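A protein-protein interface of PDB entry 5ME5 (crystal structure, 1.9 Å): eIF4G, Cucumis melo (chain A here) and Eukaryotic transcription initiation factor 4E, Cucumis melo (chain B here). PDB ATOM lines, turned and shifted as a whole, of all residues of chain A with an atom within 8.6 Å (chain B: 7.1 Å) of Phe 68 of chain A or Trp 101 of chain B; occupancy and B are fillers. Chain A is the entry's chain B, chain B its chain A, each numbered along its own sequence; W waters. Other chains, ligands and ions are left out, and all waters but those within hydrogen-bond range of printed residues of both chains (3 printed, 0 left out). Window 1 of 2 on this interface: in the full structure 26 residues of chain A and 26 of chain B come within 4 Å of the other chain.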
ATOM      1  N   SER A  57      17.886  -3.615 -14.413  1.00  0.00           N
ATOM      2  CA  SER A  57      16.449  -3.740 -14.620  1.00  0.00           C
ATOM      3  C   SER A  57      16.125  -4.885 -15.586  1.00  0.00           C
ATOM      4  O   SER A  57      16.968  -5.345 -16.357  1.00  0.00           O
ATOM      5  CB  SER A  57      15.880  -2.434 -15.182  1.00  0.00           C
ATOM      6  OG  SER A  57      16.220  -2.301 -16.565  1.00  0.00           O
ATOM      7  N   ARG A  58      14.862  -5.318 -15.566  1.00  0.00           N
ATOM      8  CA  ARG A  58      14.434  -6.377 -16.473  1.00  0.00           C
ATOM      9  C   ARG A  58      14.621  -5.961 -17.931  1.00  0.00           C
ATOM     10  O   ARG A  58      15.136  -6.733 -18.751  1.00  0.00           O
ATOM     11  CB  ARG A  58      12.972  -6.745 -16.207  1.00  0.00           C
ATOM     12  CG  ARG A  58      12.395  -7.658 -17.285  1.00  0.00           C
ATOM     13  CD  ARG A  58      10.903  -7.852 -17.143  1.00  0.00           C
ATOM     14  NE  ARG A  58      10.546  -8.206 -15.780  1.00  0.00           N
ATOM     15  CZ  ARG A  58       9.308  -8.191 -15.303  1.00  0.00           C
ATOM     16  NH1 ARG A  58       8.303  -7.832 -16.096  1.00  0.00           N
ATOM     17  NH2 ARG A  58       9.081  -8.525 -14.032  1.00  0.00           N
ATOM     18  N   ASP A  59      14.214  -4.737 -18.273  1.00  0.00           N
ATOM     19  CA  ASP A  59      14.309  -4.303 -19.668  1.00  0.00           C
ATOM     20  C   ASP A  59      15.758  -4.193 -20.113  1.00  0.00           C
ATOM     21  O   ASP A  59      16.085  -4.529 -21.256  1.00  0.00           O
ATOM     22  CB  ASP A  59      13.588  -2.973 -19.861  1.00  0.00           C
ATOM     23  CG  ASP A  59      12.092  -3.120 -19.766  1.00  0.00           C
ATOM     24  OD1 ASP A  59      11.614  -4.272 -19.848  1.00  0.00           O
ATOM     25  OD2 ASP A  59      11.392  -2.094 -19.613  1.00  0.00           O
ATOM     26  N   PHE A  60      16.649  -3.768 -19.213  1.00  0.00           N
ATOM     27  CA  PHE A  60      18.063  -3.715 -19.562  1.00  0.00           C
ATOM     28  C   PHE A  60      18.620  -5.115 -19.801  1.00  0.00           C
ATOM     29  O   PHE A  60      19.339  -5.348 -20.781  1.00  0.00           O
ATOM     30  CB  PHE A  60      18.865  -3.001 -18.470  1.00  0.00           C
ATOM     31  CG  PHE A  60      20.331  -2.858 -18.802  1.00  0.00           C
ATOM     32  CD1 PHE A  60      20.785  -1.768 -19.520  1.00  0.00           C
ATOM     33  CD2 PHE A  60      21.249  -3.822 -18.406  1.00  0.00           C
ATOM     34  CE1 PHE A  60      22.131  -1.642 -19.844  1.00  0.00           C
ATOM     35  CE2 PHE A  60      22.593  -3.704 -18.727  1.00  0.00           C
ATOM     36  CZ  PHE A  60      23.032  -2.614 -19.446  1.00  0.00           C
ATOM     37  N   LEU A  61      18.305  -6.063 -18.911  1.00  0.00           N
ATOM     38  CA  LEU A  61      18.772  -7.431 -19.111  1.00  0.00           C
ATOM     39  C   LEU A  61      18.244  -8.000 -20.420  1.00  0.00           C
ATOM     40  O   LEU A  61      18.980  -8.673 -21.157  1.00  0.00           O
ATOM     41  CB  LEU A  61      18.349  -8.312 -17.928  1.00  0.00           C
ATOM     42  CG  LEU A  61      19.121  -8.061 -16.631  1.00  0.00           C
ATOM     43  CD1 LEU A  61      18.621  -8.946 -15.475  1.00  0.00           C
ATOM     44  CD2 LEU A  61      20.599  -8.285 -16.853  1.00  0.00           C
ATOM     45  N   LEU A  62      16.979  -7.711 -20.742  1.00  0.00           N
ATOM     46  CA  LEU A  62      16.350  -8.260 -21.944  1.00  0.00           C
ATOM     47  C   LEU A  62      16.950  -7.710 -23.235  1.00  0.00           C
ATOM     48  O   LEU A  62      16.806  -8.340 -24.287  1.00  0.00           O
ATOM     49  CB  LEU A  62      14.850  -7.989 -21.936  1.00  0.00           C
ATOM     50  CG  LEU A  62      13.960  -8.813 -20.996  1.00  0.00           C
ATOM     51  CD1 LEU A  62      12.594  -8.157 -20.916  1.00  0.00           C
ATOM     52  CD2 LEU A  62      13.843 -10.247 -21.515  1.00  0.00           C
ATOM     53  N   LYS A  63      17.612  -6.556 -23.187  1.00  0.00           N
ATOM     54  CA  LYS A  63      18.222  -6.001 -24.393  1.00  0.00           C
ATOM     55  C   LYS A  63      19.311  -6.919 -24.939  1.00  0.00           C
ATOM     56  O   LYS A  63      19.587  -6.912 -26.149  1.00  0.00           O
ATOM     57  CB  LYS A  63      18.760  -4.597 -24.097  1.00  0.00           C
ATOM     58  CG  LYS A  63      20.167  -4.334 -24.595  1.00  0.00           C
ATOM     59  CD  LYS A  63      20.554  -2.867 -24.462  1.00  0.00           C
ATOM     60  CE  LYS A  63      21.271  -2.590 -23.152  1.00  0.00           C
ATOM     61  NZ  LYS A  63      22.250  -1.474 -23.309  1.00  0.00           N
ATOM     62  N   PHE A  64      19.918  -7.738 -24.076  1.00  0.00           N
ATOM     63  CA  PHE A  64      20.964  -8.654 -24.504  1.00  0.00           C
ATOM     64  C   PHE A  64      20.460 -10.024 -24.943  1.00  0.00           C
ATOM     65  O   PHE A  64      21.270 -10.823 -25.426  1.00  0.00           O
ATOM     66  CB  PHE A  64      21.972  -8.859 -23.372  1.00  0.00           C
ATOM     67  CG  PHE A  64      22.663  -7.599 -22.944  1.00  0.00           C
ATOM     68  CD1 PHE A  64      23.834  -7.199 -23.568  1.00  0.00           C
ATOM     69  CD2 PHE A  64      22.133  -6.805 -21.938  1.00  0.00           C
ATOM     70  CE1 PHE A  64      24.479  -6.039 -23.184  1.00  0.00           C
ATOM     71  CE2 PHE A  64      22.774  -5.638 -21.545  1.00  0.00           C
ATOM     72  CZ  PHE A  64      23.954  -5.256 -22.176  1.00  0.00           C
ATOM     73  N   ALA A  65      19.168 -10.335 -24.773  1.00  0.00           N
ATOM     74  CA  ALA A  65      18.740 -11.739 -24.809  1.00  0.00           C
ATOM     75  C   ALA A  65      19.012 -12.381 -26.165  1.00  0.00           C
ATOM     76  O   ALA A  65      19.545 -13.501 -26.251  1.00  0.00           O
ATOM     77  CB  ALA A  65      17.257 -11.844 -24.461  1.00  0.00           C
ATOM     78  N   GLU A  66      18.657 -11.687 -27.239  1.00  0.00           N
ATOM     79  CA  GLU A  66      18.786 -12.254 -28.579  1.00  0.00           C
ATOM     80  C   GLU A  66      20.193 -12.139 -29.147  1.00  0.00           C
ATOM     81  O   GLU A  66      20.463 -12.660 -30.239  1.00  0.00           O
ATOM     82  CB  GLU A  66      17.778 -11.578 -29.504  1.00  0.00           C
ATOM     83  CG  GLU A  66      16.454 -12.338 -29.608  1.00  0.00           C
ATOM     84  CD  GLU A  66      15.562 -12.147 -28.406  1.00  0.00           C
ATOM     85  OE1 GLU A  66      15.523 -11.010 -27.885  1.00  0.00           O
ATOM     86  OE2 GLU A  66      14.877 -13.118 -27.994  1.00  0.00           O
ATOM     87  N   GLN A  67      21.104 -11.501 -28.433  1.00  0.00           N
ATOM     88  CA  GLN A  67      22.463 -11.366 -28.924  1.00  0.00           C
ATOM     89  C   GLN A  67      23.371 -12.511 -28.491  1.00  0.00           C
ATOM     90  O   GLN A  67      24.478 -12.645 -29.028  1.00  0.00           O
ATOM     91  CB  GLN A  67      23.024 -10.015 -28.467  1.00  0.00           C
ATOM     92  CG  GLN A  67      22.049  -8.844 -28.697  1.00  0.00           C
ATOM     93  CD  GLN A  67      21.583  -8.705 -30.150  1.00  0.00           C
ATOM     94  OE1 GLN A  67      22.277  -9.116 -31.083  1.00  0.00           O
ATOM     95  NE2 GLN A  67      20.412  -8.102 -30.343  1.00  0.00           N
ATOM     96  N   PHE A  68      22.928 -13.363 -27.564  1.00  0.00           N
ATOM     97  CA  PHE A  68      23.757 -14.454 -27.045  1.00  0.00           C
ATOM     98  C   PHE A  68      22.978 -15.761 -27.136  1.00  0.00           C
ATOM     99  O   PHE A  68      22.262 -16.158 -26.208  1.00  0.00           O
ATOM    100  CB  PHE A  68      24.225 -14.116 -25.632  1.00  0.00           C
ATOM    101  CG  PHE A  68      25.124 -12.923 -25.624  1.00  0.00           C
ATOM    102  CD1 PHE A  68      26.476 -13.071 -25.902  1.00  0.00           C
ATOM    103  CD2 PHE A  68      24.601 -11.647 -25.474  1.00  0.00           C
ATOM    104  CE1 PHE A  68      27.309 -11.976 -25.968  1.00  0.00           C
ATOM    105  CE2 PHE A  68      25.428 -10.543 -25.543  1.00  0.00           C
ATOM    106  CZ  PHE A  68      26.787 -10.713 -25.799  1.00  0.00           C
ATOM    107  N   LEU A  69      23.111 -16.420 -28.284  1.00  0.00           N
ATOM    108  CA  LEU A  69      22.423 -17.671 -28.542  1.00  0.00           C
ATOM    109  C   LEU A  69      23.337 -18.882 -28.421  1.00  0.00           C
ATOM    110  O   LEU A  69      22.844 -20.011 -28.442  1.00  0.00           O
ATOM    111  CB  LEU A  69      21.801 -17.646 -29.944  1.00  0.00           C
ATOM    112  CG  LEU A  69      20.864 -16.481 -30.252  1.00  0.00           C
ATOM    113  CD1 LEU A  69      20.509 -16.498 -31.738  1.00  0.00           C
ATOM    114  CD2 LEU A  69      19.591 -16.598 -29.398  1.00  0.00           C
ATOM    115  N   ASP A  70      24.643 -18.678 -28.303  1.00  0.00           N
ATOM    116  CA  ASP A  70      25.608 -19.772 -28.352  1.00  0.00           C
ATOM    117  C   ASP A  70      25.945 -20.261 -26.947  1.00  0.00           C
ATOM    118  O   ASP A  70      26.302 -19.462 -26.082  1.00  0.00           O
ATOM    119  CB  ASP A  70      26.888 -19.313 -29.051  1.00  0.00           C
ATOM    120  CG  ASP A  70      26.672 -19.018 -30.529  1.00  0.00           C
ATOM    121  OD1 ASP A  70      25.745 -19.598 -31.126  1.00  0.00           O
ATOM    122  OD2 ASP A  70      27.436 -18.212 -31.091  1.00  0.00           O
ATOM    123  N   LEU A  71      25.868 -21.573 -26.741  1.00  0.00           N
ATOM    124  CA  LEU A  71      26.306 -22.155 -25.480  1.00  0.00           C
ATOM    125  C   LEU A  71      27.768 -21.802 -25.222  1.00  0.00           C
ATOM    126  O   LEU A  71      28.585 -21.827 -26.151  1.00  0.00           O
ATOM    127  CB  LEU A  71      26.133 -23.674 -25.520  1.00  0.00           C
ATOM    128  CG  LEU A  71      26.106 -24.528 -24.259  1.00  0.00           C
ATOM    129  CD1 LEU A  71      24.851 -24.271 -23.415  1.00  0.00           C
ATOM    130  CD2 LEU A  71      26.224 -26.001 -24.657  1.00  0.00           C
ATOM    131  N   PRO A  72      28.134 -21.464 -23.988  1.00  0.00           N
ATOM    132  CA  PRO A  72      29.554 -21.267 -23.679  1.00  0.00           C
ATOM    133  C   PRO A  72      30.341 -22.518 -24.029  1.00  0.00           C
ATOM    134  O   PRO A  72      29.850 -23.638 -23.887  1.00  0.00           O
ATOM    135  CB  PRO A  72      29.560 -21.002 -22.166  1.00  0.00           C
ATOM    136  CG  PRO A  72      28.175 -20.590 -21.840  1.00  0.00           C
ATOM    137  CD  PRO A  72      27.278 -21.308 -22.799  1.00  0.00           C
ATOM    138  N   SER A  86      18.010 -27.368 -24.723  1.00  0.00           N
ATOM    139  CA  SER A  86      16.993 -26.961 -25.684  1.00  0.00           C
ATOM    140  C   SER A  86      16.972 -27.902 -26.874  1.00  0.00           C
ATOM    141  O   SER A  86      17.996 -28.478 -27.256  1.00  0.00           O
ATOM    142  CB  SER A  86      17.248 -25.541 -26.200  1.00  0.00           C
ATOM    143  OG  SER A  86      17.186 -24.596 -25.168  1.00  0.00           O
ATOM    144  N   ASN A  90      22.815 -23.644 -30.000  1.00  0.00           N
ATOM    145  CA  ASN A  90      23.799 -22.980 -30.848  1.00  0.00           C
ATOM    146  C   ASN A  90      25.169 -22.961 -30.172  1.00  0.00           C
ATOM    147  O   ASN A  90      25.276 -23.220 -28.970  1.00  0.00           O
ATOM    148  CB  ASN A  90      23.362 -21.556 -31.181  1.00  0.00           C
ATOM    149  CG  ASN A  90      22.413 -21.493 -32.363  1.00  0.00           C
ATOM    150  OD1 ASN A  90      21.915 -22.514 -32.854  1.00  0.00           O
ATOM    151  ND2 ASN A  90      22.171 -20.280 -32.840  1.00  0.00           N
ATOM    152  N   PHE B  94      27.476 -19.111 -13.903  1.00  0.00           N
ATOM    153  CA  PHE B  94      27.641 -17.946 -14.762  1.00  0.00           C
ATOM    154  C   PHE B  94      27.827 -16.693 -13.919  1.00  0.00           C
ATOM    155  O   PHE B  94      27.362 -16.612 -12.777  1.00  0.00           O
ATOM    156  CB  PHE B  94      26.459 -17.762 -15.716  1.00  0.00           C
ATOM    157  CG  PHE B  94      25.140 -17.568 -15.029  1.00  0.00           C
ATOM    158  CD1 PHE B  94      24.356 -18.666 -14.698  1.00  0.00           C
ATOM    159  CD2 PHE B  94      24.663 -16.294 -14.743  1.00  0.00           C
ATOM    160  CE1 PHE B  94      23.145 -18.508 -14.069  1.00  0.00           C
ATOM    161  CE2 PHE B  94      23.433 -16.125 -14.105  1.00  0.00           C
ATOM    162  CZ  PHE B  94      22.671 -17.229 -13.782  1.00  0.00           C
ATOM    163  N   THR B  96      28.074 -13.299 -15.697  1.00  0.00           N
ATOM    164  CA  THR B  96      27.764 -12.098 -16.461  1.00  0.00           C
ATOM    165  C   THR B  96      26.383 -12.217 -17.097  1.00  0.00           C
ATOM    166  O   THR B  96      25.816 -13.311 -17.224  1.00  0.00           O
ATOM    167  CB  THR B  96      28.809 -11.830 -17.560  1.00  0.00           C
ATOM    168  OG1 THR B  96      28.651 -12.795 -18.603  1.00  0.00           O
ATOM    169  CG2 THR B  96      30.236 -11.929 -17.004  1.00  0.00           C
ATOM    170  N   VAL B  97      25.844 -11.060 -17.482  1.00  0.00           N
ATOM    171  CA  VAL B  97      24.595 -11.014 -18.237  1.00  0.00           C
ATOM    172  C   VAL B  97      24.729 -11.811 -19.523  1.00  0.00           C
ATOM    173  O   VAL B  97      23.838 -12.583 -19.889  1.00  0.00           O
ATOM    174  CB  VAL B  97      24.221  -9.545 -18.513  1.00  0.00           C
ATOM    175  CG1 VAL B  97      23.018  -9.430 -19.429  1.00  0.00           C
ATOM    176  CG2 VAL B  97      24.014  -8.795 -17.184  1.00  0.00           C
ATOM    177  N   GLU B  98      25.854 -11.644 -20.226  1.00  0.00           N
ATOM    178  CA  GLU B  98      26.058 -12.362 -21.475  1.00  0.00           C
ATOM    179  C   GLU B  98      26.122 -13.869 -21.249  1.00  0.00           C
ATOM    180  O   GLU B  98      25.575 -14.647 -22.044  1.00  0.00           O
ATOM    181  CB  GLU B  98      27.334 -11.851 -22.154  1.00  0.00           C
ATOM    182  CG  GLU B  98      27.245 -10.383 -22.570  1.00  0.00           C
ATOM    183  CD  GLU B  98      27.554  -9.383 -21.453  1.00  0.00           C
ATOM    184  OE1 GLU B  98      27.800  -9.807 -20.304  1.00  0.00           O
ATOM    185  OE2 GLU B  98      27.515  -8.164 -21.730  1.00  0.00           O
ATOM    186  N   GLU B  99      26.766 -14.307 -20.162  1.00  0.00           N
ATOM    187  CA  GLU B  99      26.801 -15.741 -19.875  1.00  0.00           C
ATOM    188  C   GLU B  99      25.418 -16.258 -19.491  1.00  0.00           C
ATOM    189  O   GLU B  99      25.041 -17.377 -19.862  1.00  0.00           O
ATOM    190  CB  GLU B  99      27.789 -16.048 -18.749  1.00  0.00           C
ATOM    191  CG  GLU B  99      29.246 -16.013 -19.160  1.00  0.00           C
ATOM    192  CD  GLU B  99      30.170 -16.381 -18.011  1.00  0.00           C
ATOM    193  OE1 GLU B  99      29.683 -16.504 -16.868  1.00  0.00           O
ATOM    194  OE2 GLU B  99      31.386 -16.530 -18.248  1.00  0.00           O
ATOM    195  N   PHE B 100      24.654 -15.469 -18.734  1.00  0.00           N
ATOM    196  CA  PHE B 100      23.292 -15.890 -18.398  1.00  0.00           C
ATOM    197  C   PHE B 100      22.490 -16.231 -19.651  1.00  0.00           C
ATOM    198  O   PHE B 100      21.891 -17.308 -19.751  1.00  0.00           O
ATOM    199  CB  PHE B 100      22.556 -14.807 -17.617  1.00  0.00           C
ATOM    200  CG  PHE B 100      21.085 -15.094 -17.494  1.00  0.00           C
ATOM    201  CD1 PHE B 100      20.643 -16.075 -16.626  1.00  0.00           C
ATOM    202  CD2 PHE B 100      20.160 -14.438 -18.295  1.00  0.00           C
ATOM    203  CE1 PHE B 100      19.294 -16.391 -16.535  1.00  0.00           C
ATOM    204  CE2 PHE B 100      18.807 -14.746 -18.208  1.00  0.00           C
ATOM    205  CZ  PHE B 100      18.377 -15.710 -17.333  1.00  0.00           C
ATOM    206  N   TRP B 101      22.440 -15.307 -20.615  1.00  0.00           N
ATOM    207  CA  TRP B 101      21.624 -15.563 -21.799  1.00  0.00           C
ATOM    208  C   TRP B 101      22.188 -16.723 -22.610  1.00  0.00           C
ATOM    209  O   TRP B 101      21.424 -17.525 -23.166  1.00  0.00           O
ATOM    210  CB  TRP B 101      21.493 -14.283 -22.648  1.00  0.00           C
ATOM    211  CG  TRP B 101      20.573 -13.246 -21.974  1.00  0.00           C
ATOM    212  CD1 TRP B 101      20.936 -12.026 -21.460  1.00  0.00           C
ATOM    213  CD2 TRP B 101      19.166 -13.370 -21.744  1.00  0.00           C
ATOM    214  NE1 TRP B 101      19.842 -11.389 -20.923  1.00  0.00           N
ATOM    215  CE2 TRP B 101      18.741 -12.191 -21.084  1.00  0.00           C
ATOM    216  CE3 TRP B 101      18.219 -14.358 -22.035  1.00  0.00           C
ATOM    217  CZ2 TRP B 101      17.414 -11.978 -20.715  1.00  0.00           C
ATOM    218  CZ3 TRP B 101      16.896 -14.148 -21.660  1.00  0.00           C
ATOM    219  CH2 TRP B 101      16.506 -12.968 -21.003  1.00  0.00           C
ATOM    220  N   SER B 102      23.522 -16.839 -22.673  1.00  0.00           N
ATOM    221  CA  SER B 102      24.149 -17.941 -23.412  1.00  0.00           C
ATOM    222  C   SER B 102      23.658 -19.297 -22.921  1.00  0.00           C
ATOM    223  O   SER B 102      23.468 -20.230 -23.712  1.00  0.00           O
ATOM    224  CB  SER B 102      25.675 -17.869 -23.284  1.00  0.00           C
ATOM    225  OG  SER B 102      26.177 -16.671 -23.853  1.00  0.00           O
ATOM    226  N   VAL B 103      23.451 -19.429 -21.615  1.00  0.00           N
ATOM    227  CA  VAL B 103      22.976 -20.684 -21.054  1.00  0.00           C
ATOM    228  C   VAL B 103      21.463 -20.780 -21.110  1.00  0.00           C
ATOM    229  O   VAL B 103      20.914 -21.803 -21.539  1.00  0.00           O
ATOM    230  CB  VAL B 103      23.497 -20.842 -19.610  1.00  0.00           C
ATOM    231  CG1 VAL B 103      22.800 -22.053 -18.937  1.00  0.00           C
ATOM    232  CG2 VAL B 103      25.021 -20.983 -19.628  1.00  0.00           C
ATOM    233  N   TYR B 104      20.780 -19.704 -20.690  1.00  0.00           N
ATOM    234  CA  TYR B 104      19.323 -19.711 -20.646  1.00  0.00           C
ATOM    235  C   TYR B 104      18.721 -19.996 -22.019  1.00  0.00           C
ATOM    236  O   TYR B 104      17.720 -20.723 -22.131  1.00  0.00           O
ATOM    237  CB  TYR B 104      18.822 -18.372 -20.097  1.00  0.00           C
ATOM    238  CG  TYR B 104      17.321 -18.277 -20.119  1.00  0.00           C
ATOM    239  CD1 TYR B 104      16.651 -17.803 -21.249  1.00  0.00           C
ATOM    240  CD2 TYR B 104      16.563 -18.677 -19.016  1.00  0.00           C
ATOM    241  CE1 TYR B 104      15.266 -17.738 -21.284  1.00  0.00           C
ATOM    242  CE2 TYR B 104      15.186 -18.622 -19.045  1.00  0.00           C
ATOM    243  CZ  TYR B 104      14.537 -18.139 -20.174  1.00  0.00           C
ATOM    244  OH  TYR B 104      13.158 -18.070 -20.196  1.00  0.00           O
ATOM    245  N   ASN B 105      19.307 -19.430 -23.079  1.00  0.00           N
ATOM    246  CA  ASN B 105      18.788 -19.660 -24.430  1.00  0.00           C
ATOM    247  C   ASN B 105      19.066 -21.056 -24.960  1.00  0.00           C
ATOM    248  O   ASN B 105      18.643 -21.364 -26.089  1.00  0.00           O
ATOM    249  CB  ASN B 105      19.379 -18.629 -25.395  1.00  0.00           C
ATOM    250  CG  ASN B 105      18.688 -17.302 -25.288  1.00  0.00           C
ATOM    251  OD1 ASN B 105      17.493 -17.252 -25.008  1.00  0.00           O
ATOM    252  ND2 ASN B 105      19.424 -16.223 -25.501  1.00  0.00           N
ATOM    253  N   ASN B 106      19.775 -21.902 -24.205  1.00  0.00           N
ATOM    254  CA  ASN B 106      20.093 -23.246 -24.665  1.00  0.00           C
ATOM    255  C   ASN B 106      19.620 -24.343 -23.725  1.00  0.00           C
ATOM    256  O   ASN B 106      19.947 -25.516 -23.958  1.00  0.00           O
ATOM    257  CB  ASN B 106      21.595 -23.364 -24.907  1.00  0.00           C
ATOM    258  CG  ASN B 106      21.996 -22.670 -26.189  1.00  0.00           C
ATOM    259  OD1 ASN B 106      21.656 -23.134 -27.277  1.00  0.00           O
ATOM    260  ND2 ASN B 106      22.638 -21.517 -26.072  1.00  0.00           N
ATOM    261  N   ILE B 107      18.855 -24.007 -22.684  1.00  0.00           N
ATOM    262  CA  ILE B 107      18.226 -25.016 -21.846  1.00  0.00           C
ATOM    263  C   ILE B 107      16.715 -24.852 -21.948  1.00  0.00           C
ATOM    264  O   ILE B 107      16.197 -23.770 -22.255  1.00  0.00           O
ATOM    265  CB  ILE B 107      18.685 -24.954 -20.372  1.00  0.00           C
ATOM    266  CG1 ILE B 107      18.153 -23.683 -19.702  1.00  0.00           C
ATOM    267  CG2 ILE B 107      20.208 -25.097 -20.274  1.00  0.00           C
ATOM    268  CD1 ILE B 107      18.629 -23.510 -18.253  1.00  0.00           C
ATOM    269  N   LEU B 155      11.298 -16.854 -15.989  1.00  0.00           N
ATOM    270  CA  LEU B 155      12.278 -15.890 -16.508  1.00  0.00           C
ATOM    271  C   LEU B 155      12.298 -14.613 -15.670  1.00  0.00           C
ATOM    272  O   LEU B 155      13.366 -14.098 -15.318  1.00  0.00           O
ATOM    273  CB  LEU B 155      11.975 -15.544 -17.965  1.00  0.00           C
ATOM    274  CG  LEU B 155      12.841 -14.436 -18.582  1.00  0.00           C
ATOM    275  CD1 LEU B 155      14.327 -14.806 -18.546  1.00  0.00           C
ATOM    276  CD2 LEU B 155      12.410 -14.131 -20.017  1.00  0.00           C
ATOM    277  N   LEU B 159      15.504 -12.939 -13.795  1.00  0.00           N
ATOM    278  CA  LEU B 159      16.007 -11.595 -14.076  1.00  0.00           C
ATOM    279  C   LEU B 159      15.980 -10.720 -12.828  1.00  0.00           C
ATOM    280  O   LEU B 159      16.904  -9.929 -12.600  1.00  0.00           O
ATOM    281  CB  LEU B 159      15.196 -10.942 -15.195  1.00  0.00           C
ATOM    282  CG  LEU B 159      15.274 -11.668 -16.545  1.00  0.00           C
ATOM    283  CD1 LEU B 159      14.569 -10.843 -17.615  1.00  0.00           C
ATOM    284  CD2 LEU B 159      16.754 -11.939 -16.930  1.00  0.00           C
ATOM    285  N   ILE B 162      19.081 -12.091 -10.522  1.00  0.00           N
ATOM    286  CA  ILE B 162      20.458 -11.825 -10.946  1.00  0.00           C
ATOM    287  C   ILE B 162      20.689 -10.338 -11.143  1.00  0.00           C
ATOM    288  O   ILE B 162      21.837  -9.860 -11.050  1.00  0.00           O
ATOM    289  CB  ILE B 162      20.823 -12.618 -12.216  1.00  0.00           C
ATOM    290  CG1 ILE B 162      20.044 -12.093 -13.426  1.00  0.00           C
ATOM    291  CG2 ILE B 162      20.582 -14.104 -12.019  1.00  0.00           C
ATOM    292  CD1 ILE B 162      20.531 -12.683 -14.730  1.00  0.00           C
HETATM  293  O   HOH W   1      16.168  -7.450 -13.457  1.00  0.00           O
HETATM  294  O   HOH W   2      15.748 -22.525 -24.588  1.00  0.00           O
HETATM  295  O   HOH W   3      26.393 -16.610 -26.930  1.00  0.00           O
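The backbone NH of Glu 98 of chain B lies close to the side-chain hydroxyl of Thr 96 of chain B, at 3.4 Å.
The side-chain hydroxyl (OG) of Ser 102 of chain B is in hydrogen-bond range of the backbone carbonyl oxygen (O) of Glu 98 of chain B (2.8 Å).
The backbone carbonyl oxygen (O) of Trp 101 of chain B sits close to the side-chain amide nitrogen (ND2) of Asn 105 of chain B (3.3 Å).
The backbone carbonyl oxygen (O) of Ser 102 of chain B is in hydrogen-bond range of the side-chain amide nitrogen (ND2) of Asn 106 of chain B, at 2.8 Å.
O of Asn 90 of chain A lies within hydrogen-bond range of N of Leu 71 of chain A (2.8 Å).
Printed residues of chain B that touch a printed residue of chain A: Val 97, Glu 98, Trp 101, Ser 102, Val 103, Asn 105, Asn 106, Ile 107 and Leu 159.
Hydrophobic or aromatic side chains of chain B that line the printed part of chain A: Val 97, Trp 101, Val 103 and Leu 159.
Of the 18 printed residues of chain A, 12 touch a printed residue of chain B.
Hydrophobic or aromatic side chains of chain A that line the printed part of chain B: Leu 61, Leu 62, Phe 64, Ala 65, Phe 68, Leu 69, Leu 71 and Pro 72.
Among the printed residues, 27 pairs touch across the chains.
Among the printed residues, no Asp or Glu carboxylate lies within 4 Å of a Lys or Arg side-chain nitrogen of the other chain.
The indole nitrogen of Trp 101 of chain B is in hydrogen-bond range of the backbone carbonyl oxygen of Leu 61 of chain A, at 2.9 Å.
The side-chain amide nitrogen (ND2) of Asn 105 of chain B lies within hydrogen-bond range of the backbone carbonyl oxygen (O) of Ala 65 of chain A (2.8 Å).
ND2 of Asn 105 of chain B is in hydrogen-bond range of O of Phe 68 of chain A, 2.9 Å away.
The side-chain amide nitrogen (ND2) of Asn 106 of chain B sits at hydrogen-bond distance from the backbone carbonyl oxygen (O) of Leu 69 of chain A (2.8 Å).
The side-chain amide nitrogen of Asn 106 of chain B lies close to the backbone NH of Leu 71 of chain A (3.3 Å).
The backbone carbonyl oxygen (O) of Asn 106 of chain B is in hydrogen-bond range of the backbone NH (N) of Ser 86 of chain A, at 2.8 Å.
OD1 of Asn 106 of chain B is in hydrogen-bond range of N of Asn 90 of chain A (3.0 Å).
N of Ile 107 of chain B is in hydrogen-bond range of OG of Ser 86 of chain A (3.1 Å).
The backbone carbonyl oxygen (O) of Phe 68 of chain A lies close to the backbone carbonyl oxygen (O) of Trp 101 of chain B (3.4 Å).
Arg 58 of chain A touches Leu 159 of chain B (CG to CD1, 3.9 Å).
Leu 62 of chain A touches Leu 159 of chain B (CG to CD1, 3.99 Å).
Glu 98 of chain B touches Phe 64 of chain A (OE2 to CE1, 3.98 Å).
Phe 64 of chain A touches Trp 101 of chain B (CB to CD1, 3.8 Å).
Trp 101 of chain B touches Ala 65 of chain A.
Phe 68 of chain A touches Glu 98 of chain B.
Asp 70 of chain A touches Ser 102 of chain B (O to CB, 3.3 Å).
Pro 72 of chain A touches Ser 102 of chain B.
Pro 72 of chain A touches Val 103 of chain B (CG to CG2, 3.9 Å).
Asn 105 of chain B touches Ser 86 of chain A.
Water W2 lies within hydrogen-bond range of OG of Ser 86 of chain A (2.6 Å), O of Ile 107 of chain B (2.7 Å) and O of Asn 105 of chain B (3.5 Å).
Water W1 lies within hydrogen-bond range of O of Leu 159 of chain B (2.7 Å) and N of Arg 58 of chain A (3.3 Å).
Water W3 lies within hydrogen-bond range of the backbone carbonyl oxygen of Asp 70 of chain A (3.0 Å) and the side-chain hydroxyl of Ser 102 of chain B (3.1 Å).
Asp 59 of chain A touches none of the printed residues of chain B.
Of the printed residues of chain B, Ala 65 of chain A touches Trp 101 and Asn 105.
Of chain B, only Glu 98, Trp 101, Ser 102 and Asn 105 come within 4 Å of Phe 68 of chain A.
Of the printed residues of chain B, Asp 70 of chain A touches Ser 102 and Asn 106.
The nearest residue of chain B that does not touch Phe 68 of chain A is Asn 106 of chain B (5.4 Å).
The nearest residue of chain A that does not touch Trp 101 of chain B is Leu 69 of chain A (5.5 Å).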
